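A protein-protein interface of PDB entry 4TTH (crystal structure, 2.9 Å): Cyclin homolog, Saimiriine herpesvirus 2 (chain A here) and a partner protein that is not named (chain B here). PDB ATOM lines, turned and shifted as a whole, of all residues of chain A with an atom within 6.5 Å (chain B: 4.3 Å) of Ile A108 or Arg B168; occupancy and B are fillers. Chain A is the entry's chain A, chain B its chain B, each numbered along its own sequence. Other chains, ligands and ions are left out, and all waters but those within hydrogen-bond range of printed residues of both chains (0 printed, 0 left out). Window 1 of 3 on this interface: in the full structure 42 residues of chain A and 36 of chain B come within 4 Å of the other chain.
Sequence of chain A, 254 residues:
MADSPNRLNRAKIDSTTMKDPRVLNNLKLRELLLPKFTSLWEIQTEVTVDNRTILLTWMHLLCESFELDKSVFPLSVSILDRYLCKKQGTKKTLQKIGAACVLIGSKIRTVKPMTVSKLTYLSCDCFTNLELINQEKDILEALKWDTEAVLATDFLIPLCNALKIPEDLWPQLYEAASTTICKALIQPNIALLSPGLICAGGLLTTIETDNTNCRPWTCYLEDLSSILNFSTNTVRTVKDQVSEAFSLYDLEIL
The side-chain carboxylate of Asp A69 is in hydrogen-bond range of the backbone NH of Ala B175. NE of Arg B60 is in hydrogen-bond range of O of Lys A107, 3.1 Å away. NE of Arg B60 lies within hydrogen-bond range of O of Ile A108, 3.2 Å away. O of Arg A109 lies within hydrogen-bond range of NH2 of Arg B168 (3.3 Å). The backbone carbonyl oxygen (O) of Thr A110 lies within hydrogen-bond range of the guanidinium group (NH2) of Arg B60, at 3.3 Å.
OG1 of Thr A110 is in hydrogen-bond range of OD1 of Asp A69 (3.0 Å). NH2 of Arg A109 is in salt-bridge range of OE1 of Glu A148. The backbone carbonyl oxygen (O) of Arg B168 sits at hydrogen-bond distance from the backbone NH (N) of Val B142 (3.3 Å).
Among the printed residues, pairs that only touch across the chains: Asp A69 with Met B174, Ile A108 with Ile B59, Ile A108 with Arg B168, Arg A109 with Ile B169, Thr A110 with Arg B168, Val A111 with Ala B175 and Glu A148 with Ile B169.
Of the printed residues of chain B, Lys A107 touches Arg B60. Ile A108 touches just these residues of chain B: Ile B59 (3.9 Å), Arg B60 (3.2 Å) and Arg B168 (3.5 Å). Of the printed residues of chain A, Arg B60 touches Lys A107, Ile A108 and Thr A110. Arg B168 touches just these residues of chain A: Ile A108, Arg A109 and Thr A110. The nearest residue of chain A that does not touch Arg B168 is Val A111 (4.05 Å). The nearest printed residue of chain A that does not touch Ala B175 is Thr A110 (5.8 Å).
Printed residues of chain B that touch a printed residue of chain A: Ile B59, Arg B60, Arg B168, Ile B169, Met B174 and Ala B175. Hydrophobic or aromatic side chains of chain B that line the printed part of chain A: Ile B59, Ile B169, Met B174 and Ala B175. Printed residues of chain A that touch a printed residue of chain B: Asp A69, Lys A107, Ile A108, Arg A109, Thr A110, Val A111 and Glu A148. Hydrophobic or aromatic side chains of chain A within 4 Å of the printed part of chain B: Ile A108 and Val A111. Among the printed residues, 12 pairs touch across the chains. Among the printed residues, no Asp or Glu carboxylate lies within 4 Å of a Lys or Arg side-chain nitrogen of the other chain.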
ATOM      1  N   ASP A  69       1.041  16.868  11.545  1.00  0.00           N
ATOM      2  CA  ASP A  69       0.476  18.161  11.951  1.00  0.00           C
ATOM      3  C   ASP A  69       1.479  18.926  12.797  1.00  0.00           C
ATOM      4  O   ASP A  69       2.190  18.315  13.606  1.00  0.00           O
ATOM      5  CB  ASP A  69      -0.821  17.956  12.737  1.00  0.00           C
ATOM      6  CG  ASP A  69      -2.039  17.723  11.837  1.00  0.00           C
ATOM      7  OD1 ASP A  69      -2.832  16.789  12.125  1.00  0.00           O
ATOM      8  OD2 ASP A  69      -2.221  18.492  10.866  1.00  0.00           O
ATOM      9  N   LEU A  75       4.489  18.545  21.243  1.00  0.00           N
ATOM     10  CA  LEU A  75       3.999  17.619  22.256  1.00  0.00           C
ATOM     11  C   LEU A  75       5.000  16.515  22.568  1.00  0.00           C
ATOM     12  O   LEU A  75       5.193  16.158  23.732  1.00  0.00           O
ATOM     13  CB  LEU A  75       2.635  17.026  21.894  1.00  0.00           C
ATOM     14  CG  LEU A  75       2.039  16.035  22.908  1.00  0.00           C
ATOM     15  CD1 LEU A  75       1.980  16.659  24.288  1.00  0.00           C
ATOM     16  CD2 LEU A  75       0.653  15.594  22.491  1.00  0.00           C
ATOM     17  N   ILE A  79       6.405  15.772  26.248  1.00  0.00           N
ATOM     18  CA  ILE A  79       6.376  14.429  26.826  1.00  0.00           C
ATOM     19  C   ILE A  79       7.747  13.931  27.223  1.00  0.00           C
ATOM     20  O   ILE A  79       7.927  13.405  28.299  1.00  0.00           O
ATOM     21  CB  ILE A  79       5.844  13.365  25.842  1.00  0.00           C
ATOM     22  CG1 ILE A  79       4.394  13.611  25.453  1.00  0.00           C
ATOM     23  CG2 ILE A  79       5.941  11.983  26.449  1.00  0.00           C
ATOM     24  CD1 ILE A  79       3.775  12.444  24.723  1.00  0.00           C
ATOM     25  N   LEU A 103       5.396   8.393  19.033  1.00  0.00           N
ATOM     26  CA  LEU A 103       4.299   7.454  18.907  1.00  0.00           C
ATOM     27  C   LEU A 103       3.088   7.961  19.684  1.00  0.00           C
ATOM     28  O   LEU A 103       1.972   7.991  19.159  1.00  0.00           O
ATOM     29  CB  LEU A 103       4.694   6.064  19.390  1.00  0.00           C
ATOM     30  CG  LEU A 103       3.517   5.119  19.167  1.00  0.00           C
ATOM     31  CD1 LEU A 103       3.069   5.171  17.709  1.00  0.00           C
ATOM     32  CD2 LEU A 103       3.853   3.698  19.603  1.00  0.00           C
ATOM     33  N   ILE A 104       3.320   8.376  20.930  1.00  0.00           N
ATOM     34  CA  ILE A 104       2.246   8.880  21.785  1.00  0.00           C
ATOM     35  C   ILE A 104       1.695  10.206  21.269  1.00  0.00           C
ATOM     36  O   ILE A 104       0.491  10.368  21.118  1.00  0.00           O
ATOM     37  CB  ILE A 104       2.711   9.074  23.246  1.00  0.00           C
ATOM     38  CG1 ILE A 104       3.170   7.755  23.871  1.00  0.00           C
ATOM     39  CG2 ILE A 104       1.593   9.656  24.075  1.00  0.00           C
ATOM     40  CD1 ILE A 104       3.937   7.954  25.152  1.00  0.00           C
ATOM     41  N   GLY A 105       2.590  11.145  20.990  1.00  0.00           N
ATOM     42  CA  GLY A 105       2.202  12.479  20.570  1.00  0.00           C
ATOM     43  C   GLY A 105       1.411  12.539  19.284  1.00  0.00           C
ATOM     44  O   GLY A 105       0.615  13.451  19.082  1.00  0.00           O
ATOM     45  N   SER A 106       1.641  11.563  18.409  1.00  0.00           N
ATOM     46  CA  SER A 106       0.947  11.471  17.130  1.00  0.00           C
ATOM     47  C   SER A 106      -0.476  11.002  17.328  1.00  0.00           C
ATOM     48  O   SER A 106      -1.391  11.451  16.653  1.00  0.00           O
ATOM     49  CB  SER A 106       1.665  10.468  16.228  1.00  0.00           C
ATOM     50  OG  SER A 106       2.093   9.347  16.982  1.00  0.00           O
ATOM     51  N   LYS A 107      -0.633  10.068  18.257  1.00  0.00           N
ATOM     52  CA  LYS A 107      -1.914   9.458  18.550  1.00  0.00           C
ATOM     53  C   LYS A 107      -2.848  10.513  19.081  1.00  0.00           C
ATOM     54  O   LYS A 107      -4.057  10.463  18.869  1.00  0.00           O
ATOM     55  CB  LYS A 107      -1.729   8.330  19.563  1.00  0.00           C
ATOM     56  CG  LYS A 107      -1.074   7.100  18.953  1.00  0.00           C
ATOM     57  CD  LYS A 107      -0.609   6.122  20.002  1.00  0.00           C
ATOM     58  CE  LYS A 107      -0.762   4.695  19.513  1.00  0.00           C
ATOM     59  NZ  LYS A 107      -0.158   3.735  20.470  1.00  0.00           N
ATOM     60  N   ILE A 108      -2.269  11.502  19.741  1.00  0.00           N
ATOM     61  CA  ILE A 108      -3.065  12.589  20.287  1.00  0.00           C
ATOM     62  C   ILE A 108      -3.317  13.711  19.285  1.00  0.00           C
ATOM     63  O   ILE A 108      -4.462  14.007  18.985  1.00  0.00           O
ATOM     64  CB  ILE A 108      -2.460  13.155  21.575  1.00  0.00           C
ATOM     65  CG1 ILE A 108      -2.530  12.112  22.685  1.00  0.00           C
ATOM     66  CG2 ILE A 108      -3.210  14.372  21.968  1.00  0.00           C
ATOM     67  CD1 ILE A 108      -1.403  12.183  23.635  1.00  0.00           C
ATOM     68  N   ARG A 109      -2.270  14.319  18.744  1.00  0.00           N
ATOM     69  CA  ARG A 109      -2.467  15.556  17.995  1.00  0.00           C
ATOM     70  C   ARG A 109      -2.577  15.444  16.475  1.00  0.00           C
ATOM     71  O   ARG A 109      -2.680  16.477  15.800  1.00  0.00           O
ATOM     72  CB  ARG A 109      -1.388  16.575  18.362  1.00  0.00           C
ATOM     73  CG  ARG A 109      -1.495  17.121  19.800  1.00  0.00           C
ATOM     74  CD  ARG A 109      -2.571  18.208  19.965  1.00  0.00           C
ATOM     75  NE  ARG A 109      -2.403  18.869  21.251  1.00  0.00           N
ATOM     76  CZ  ARG A 109      -2.118  20.158  21.396  1.00  0.00           C
ATOM     77  NH1 ARG A 109      -2.006  20.939  20.335  1.00  0.00           N
ATOM     78  NH2 ARG A 109      -1.955  20.672  22.604  1.00  0.00           N
ATOM     79  N   THR A 110      -2.558  14.215  15.948  1.00  0.00           N
ATOM     80  CA  THR A 110      -2.569  13.971  14.495  1.00  0.00           C
ATOM     81  C   THR A 110      -3.502  12.821  14.125  1.00  0.00           C
ATOM     82  O   THR A 110      -3.620  11.828  14.856  1.00  0.00           O
ATOM     83  CB  THR A 110      -1.124  13.717  13.911  1.00  0.00           C
ATOM     84  OG1 THR A 110      -0.887  14.564  12.774  1.00  0.00           O
ATOM     85  CG2 THR A 110      -0.916  12.271  13.509  1.00  0.00           C
ATOM     86  N   VAL A 111      -4.161  12.956  12.980  1.00  0.00           N
ATOM     87  CA  VAL A 111      -5.225  12.031  12.602  1.00  0.00           C
ATOM     88  C   VAL A 111      -4.736  10.655  12.110  1.00  0.00           C
ATOM     89  O   VAL A 111      -5.347   9.628  12.420  1.00  0.00           O
ATOM     90  CB  VAL A 111      -6.178  12.678  11.598  1.00  0.00           C
ATOM     91  CG1 VAL A 111      -5.480  12.922  10.296  1.00  0.00           C
ATOM     92  CG2 VAL A 111      -7.354  11.797  11.397  1.00  0.00           C
ATOM     93  N   THR A 147      -0.761  13.310  29.536  1.00  0.00           N
ATOM     94  CA  THR A 147       0.142  13.386  28.407  1.00  0.00           C
ATOM     95  C   THR A 147       0.052  14.697  27.684  1.00  0.00           C
ATOM     96  O   THR A 147       1.072  15.221  27.232  1.00  0.00           O
ATOM     97  CB  THR A 147      -0.099  12.251  27.426  1.00  0.00           C
ATOM     98  OG1 THR A 147      -1.505  12.089  27.226  1.00  0.00           O
ATOM     99  CG2 THR A 147       0.478  10.959  27.983  1.00  0.00           C
ATOM    100  N   GLU A 148      -1.157  15.236  27.584  1.00  0.00           N
ATOM    101  CA  GLU A 148      -1.354  16.479  26.853  1.00  0.00           C
ATOM    102  C   GLU A 148      -0.627  17.612  27.600  1.00  0.00           C
ATOM    103  O   GLU A 148      -0.058  17.392  28.673  1.00  0.00           O
ATOM    104  CB  GLU A 148      -2.846  16.731  26.616  1.00  0.00           C
ATOM    105  CG  GLU A 148      -3.198  17.910  25.725  1.00  0.00           C
ATOM    106  CD  GLU A 148      -2.516  17.883  24.346  1.00  0.00           C
ATOM    107  OE1 GLU A 148      -1.462  18.547  24.186  1.00  0.00           O
ATOM    108  OE2 GLU A 148      -3.057  17.240  23.412  1.00  0.00           O
ATOM    109  N   ILE B  59      -6.119   6.822  24.765  1.00  0.00           N
ATOM    110  CA  ILE B  59      -5.016   7.728  25.066  1.00  0.00           C
ATOM    111  C   ILE B  59      -5.454   9.174  24.895  1.00  0.00           C
ATOM    112  O   ILE B  59      -5.106  10.029  25.695  1.00  0.00           O
ATOM    113  CB  ILE B  59      -3.777   7.446  24.190  1.00  0.00           C
ATOM    114  CG1 ILE B  59      -3.089   6.159  24.639  1.00  0.00           C
ATOM    115  CG2 ILE B  59      -2.784   8.605  24.257  1.00  0.00           C
ATOM    116  CD1 ILE B  59      -1.741   5.945  23.992  1.00  0.00           C
ATOM    117  N   ARG B  60      -6.234   9.443  23.858  1.00  0.00           N
ATOM    118  CA  ARG B  60      -6.831  10.759  23.675  1.00  0.00           C
ATOM    119  C   ARG B  60      -7.789  11.124  24.804  1.00  0.00           C
ATOM    120  O   ARG B  60      -7.675  12.193  25.401  1.00  0.00           O
ATOM    121  CB  ARG B  60      -7.596  10.810  22.363  1.00  0.00           C
ATOM    122  CG  ARG B  60      -6.734  11.103  21.184  1.00  0.00           C
ATOM    123  CD  ARG B  60      -7.583  11.271  19.941  1.00  0.00           C
ATOM    124  NE  ARG B  60      -6.801  11.831  18.845  1.00  0.00           N
ATOM    125  CZ  ARG B  60      -7.088  11.649  17.567  1.00  0.00           C
ATOM    126  NH1 ARG B  60      -8.147  10.927  17.222  1.00  0.00           N
ATOM    127  NH2 ARG B  60      -6.324  12.207  16.636  1.00  0.00           N
ATOM    128  N   ARG B 140     -10.202  24.848  23.825  1.00  0.00           N
ATOM    129  CA  ARG B 140      -9.921  24.431  22.468  1.00  0.00           C
ATOM    130  C   ARG B 140     -10.164  22.941  22.297  1.00  0.00           C
ATOM    131  O   ARG B 140      -9.514  22.299  21.494  1.00  0.00           O
ATOM    132  CB  ARG B 140      -8.493  24.813  22.070  1.00  0.00           C
ATOM    133  CG  ARG B 140      -8.209  26.313  22.056  1.00  0.00           C
ATOM    134  CD  ARG B 140      -6.987  26.629  21.211  1.00  0.00           C
ATOM    135  NE  ARG B 140      -6.085  25.477  21.209  1.00  0.00           N
ATOM    136  CZ  ARG B 140      -5.156  25.241  20.283  1.00  0.00           C
ATOM    137  NH1 ARG B 140      -4.988  26.081  19.269  1.00  0.00           N
ATOM    138  NH2 ARG B 140      -4.389  24.159  20.370  1.00  0.00           N
ATOM    139  N   VAL B 141     -11.105  22.395  23.059  1.00  0.00           N
ATOM    140  CA  VAL B 141     -11.466  20.987  22.938  1.00  0.00           C
ATOM    141  C   VAL B 141     -12.821  20.852  22.255  1.00  0.00           C
ATOM    142  O   VAL B 141     -13.731  21.639  22.518  1.00  0.00           O
ATOM    143  CB  VAL B 141     -11.516  20.297  24.308  1.00  0.00           C
ATOM    144  CG1 VAL B 141     -12.092  18.886  24.189  1.00  0.00           C
ATOM    145  CG2 VAL B 141     -10.131  20.265  24.916  1.00  0.00           C
ATOM    146  N   VAL B 142     -12.956  19.877  21.355  1.00  0.00           N
ATOM    147  CA  VAL B 142     -14.270  19.578  20.779  1.00  0.00           C
ATOM    148  C   VAL B 142     -14.684  18.159  21.148  1.00  0.00           C
ATOM    149  O   VAL B 142     -13.901  17.224  21.004  1.00  0.00           O
ATOM    150  CB  VAL B 142     -14.338  19.814  19.251  1.00  0.00           C
ATOM    151  CG1 VAL B 142     -15.773  19.918  18.804  1.00  0.00           C
ATOM    152  CG2 VAL B 142     -13.644  21.099  18.880  1.00  0.00           C
ATOM    153  N   ARG B 144     -16.877  15.520  19.997  1.00  0.00           N
ATOM    154  CA  ARG B 144     -17.647  15.238  18.814  1.00  0.00           C
ATOM    155  C   ARG B 144     -18.158  13.833  18.906  1.00  0.00           C
ATOM    156  O   ARG B 144     -17.718  12.960  18.185  1.00  0.00           O
ATOM    157  CB  ARG B 144     -16.739  15.397  17.608  1.00  0.00           C
ATOM    158  CG  ARG B 144     -15.830  16.585  17.769  1.00  0.00           C
ATOM    159  CD  ARG B 144     -14.637  16.519  16.869  1.00  0.00           C
ATOM    160  NE  ARG B 144     -13.781  15.370  17.126  1.00  0.00           N
ATOM    161  CZ  ARG B 144     -12.767  15.029  16.328  1.00  0.00           C
ATOM    162  NH1 ARG B 144     -12.507  15.750  15.243  1.00  0.00           N
ATOM    163  NH2 ARG B 144     -12.015  13.968  16.603  1.00  0.00           N
ATOM    164  N   LEU B 166     -13.609  10.558  20.738  1.00  0.00           N
ATOM    165  CA  LEU B 166     -13.485  11.300  19.493  1.00  0.00           C
ATOM    166  C   LEU B 166     -13.069  12.714  19.773  1.00  0.00           C
ATOM    167  O   LEU B 166     -13.090  13.558  18.888  1.00  0.00           O
ATOM    168  CB  LEU B 166     -14.818  11.340  18.746  1.00  0.00           C
ATOM    169  CG  LEU B 166     -15.451   9.999  18.409  1.00  0.00           C
ATOM    170  CD1 LEU B 166     -16.561  10.165  17.365  1.00  0.00           C
ATOM    171  CD2 LEU B 166     -14.375   9.020  17.944  1.00  0.00           C
ATOM    172  N   ALA B 167     -12.728  12.988  21.021  1.00  0.00           N
ATOM    173  CA  ALA B 167     -12.470  14.358  21.424  1.00  0.00           C
ATOM    174  C   ALA B 167     -11.000  14.672  21.262  1.00  0.00           C
ATOM    175  O   ALA B 167     -10.141  13.820  21.495  1.00  0.00           O
ATOM    176  CB  ALA B 167     -12.893  14.562  22.855  1.00  0.00           C
ATOM    177  N   ARG B 168     -10.707  15.894  20.851  1.00  0.00           N
ATOM    178  CA  ARG B 168      -9.329  16.351  20.880  1.00  0.00           C
ATOM    179  C   ARG B 168      -9.200  17.858  20.777  1.00  0.00           C
ATOM    180  O   ARG B 168     -10.139  18.556  20.406  1.00  0.00           O
ATOM    181  CB  ARG B 168      -8.491  15.666  19.794  1.00  0.00           C
ATOM    182  CG  ARG B 168      -9.157  15.587  18.425  1.00  0.00           C
ATOM    183  CD  ARG B 168      -8.472  14.535  17.603  1.00  0.00           C
ATOM    184  NE  ARG B 168      -7.221  15.033  17.035  1.00  0.00           N
ATOM    185  CZ  ARG B 168      -7.047  15.311  15.747  1.00  0.00           C
ATOM    186  NH1 ARG B 168      -8.036  15.124  14.884  1.00  0.00           N
ATOM    187  NH2 ARG B 168      -5.888  15.772  15.320  1.00  0.00           N
ATOM    188  N   ILE B 169      -8.018  18.345  21.122  1.00  0.00           N
ATOM    189  CA  ILE B 169      -7.699  19.752  20.967  1.00  0.00           C
ATOM    190  C   ILE B 169      -7.682  20.155  19.493  1.00  0.00           C
ATOM    191  O   ILE B 169      -7.019  19.534  18.682  1.00  0.00           O
ATOM    192  CB  ILE B 169      -6.341  20.077  21.612  1.00  0.00           C
ATOM    193  CG1 ILE B 169      -6.301  19.477  23.008  1.00  0.00           C
ATOM    194  CG2 ILE B 169      -6.071  21.550  21.571  1.00  0.00           C
ATOM    195  CD1 ILE B 169      -5.314  20.114  23.945  1.00  0.00           C
ATOM    196  N   TYR B 170      -8.419  21.199  19.161  1.00  0.00           N
ATOM    197  CA  TYR B 170      -8.380  21.767  17.835  1.00  0.00           C
ATOM    198  C   TYR B 170      -7.354  22.874  17.681  1.00  0.00           C
ATOM    199  O   TYR B 170      -7.612  24.029  18.046  1.00  0.00           O
ATOM    200  CB  TYR B 170      -9.742  22.346  17.460  1.00  0.00           C
ATOM    201  CG  TYR B 170     -10.587  21.478  16.555  1.00  0.00           C
ATOM    202  CD1 TYR B 170     -10.927  20.182  16.918  1.00  0.00           C
ATOM    203  CD2 TYR B 170     -11.062  21.964  15.344  1.00  0.00           C
ATOM    204  CE1 TYR B 170     -11.708  19.405  16.110  1.00  0.00           C
ATOM    205  CE2 TYR B 170     -11.843  21.187  14.523  1.00  0.00           C
ATOM    206  CZ  TYR B 170     -12.174  19.910  14.919  1.00  0.00           C
ATOM    207  OH  TYR B 170     -12.965  19.117  14.102  1.00  0.00           O
ATOM    208  N   MET B 174      -5.166  21.710  10.975  1.00  0.00           N
ATOM    209  CA  MET B 174      -4.897  20.323  11.322  1.00  0.00           C
ATOM    210  C   MET B 174      -5.824  19.404  10.561  1.00  0.00           C
ATOM    211  O   MET B 174      -6.927  19.776  10.189  1.00  0.00           O
ATOM    212  CB  MET B 174      -5.068  20.079  12.817  1.00  0.00           C
ATOM    213  CG  MET B 174      -6.452  20.425  13.339  1.00  0.00           C
ATOM    214  SD  MET B 174      -6.745  19.809  14.991  1.00  0.00           S
ATOM    215  CE  MET B 174      -7.757  18.372  14.749  1.00  0.00           C
ATOM    216  N   ALA B 175      -5.355  18.189  10.334  1.00  0.00           N
ATOM    217  CA  ALA B 175      -6.082  17.228   9.533  1.00  0.00           C
ATOM    218  C   ALA B 175      -7.224  16.665  10.370  1.00  0.00           C
ATOM    219  O   ALA B 175      -7.205  16.773  11.598  1.00  0.00           O
ATOM    220  CB  ALA B 175      -5.147  16.138   9.094  1.00  0.00           C
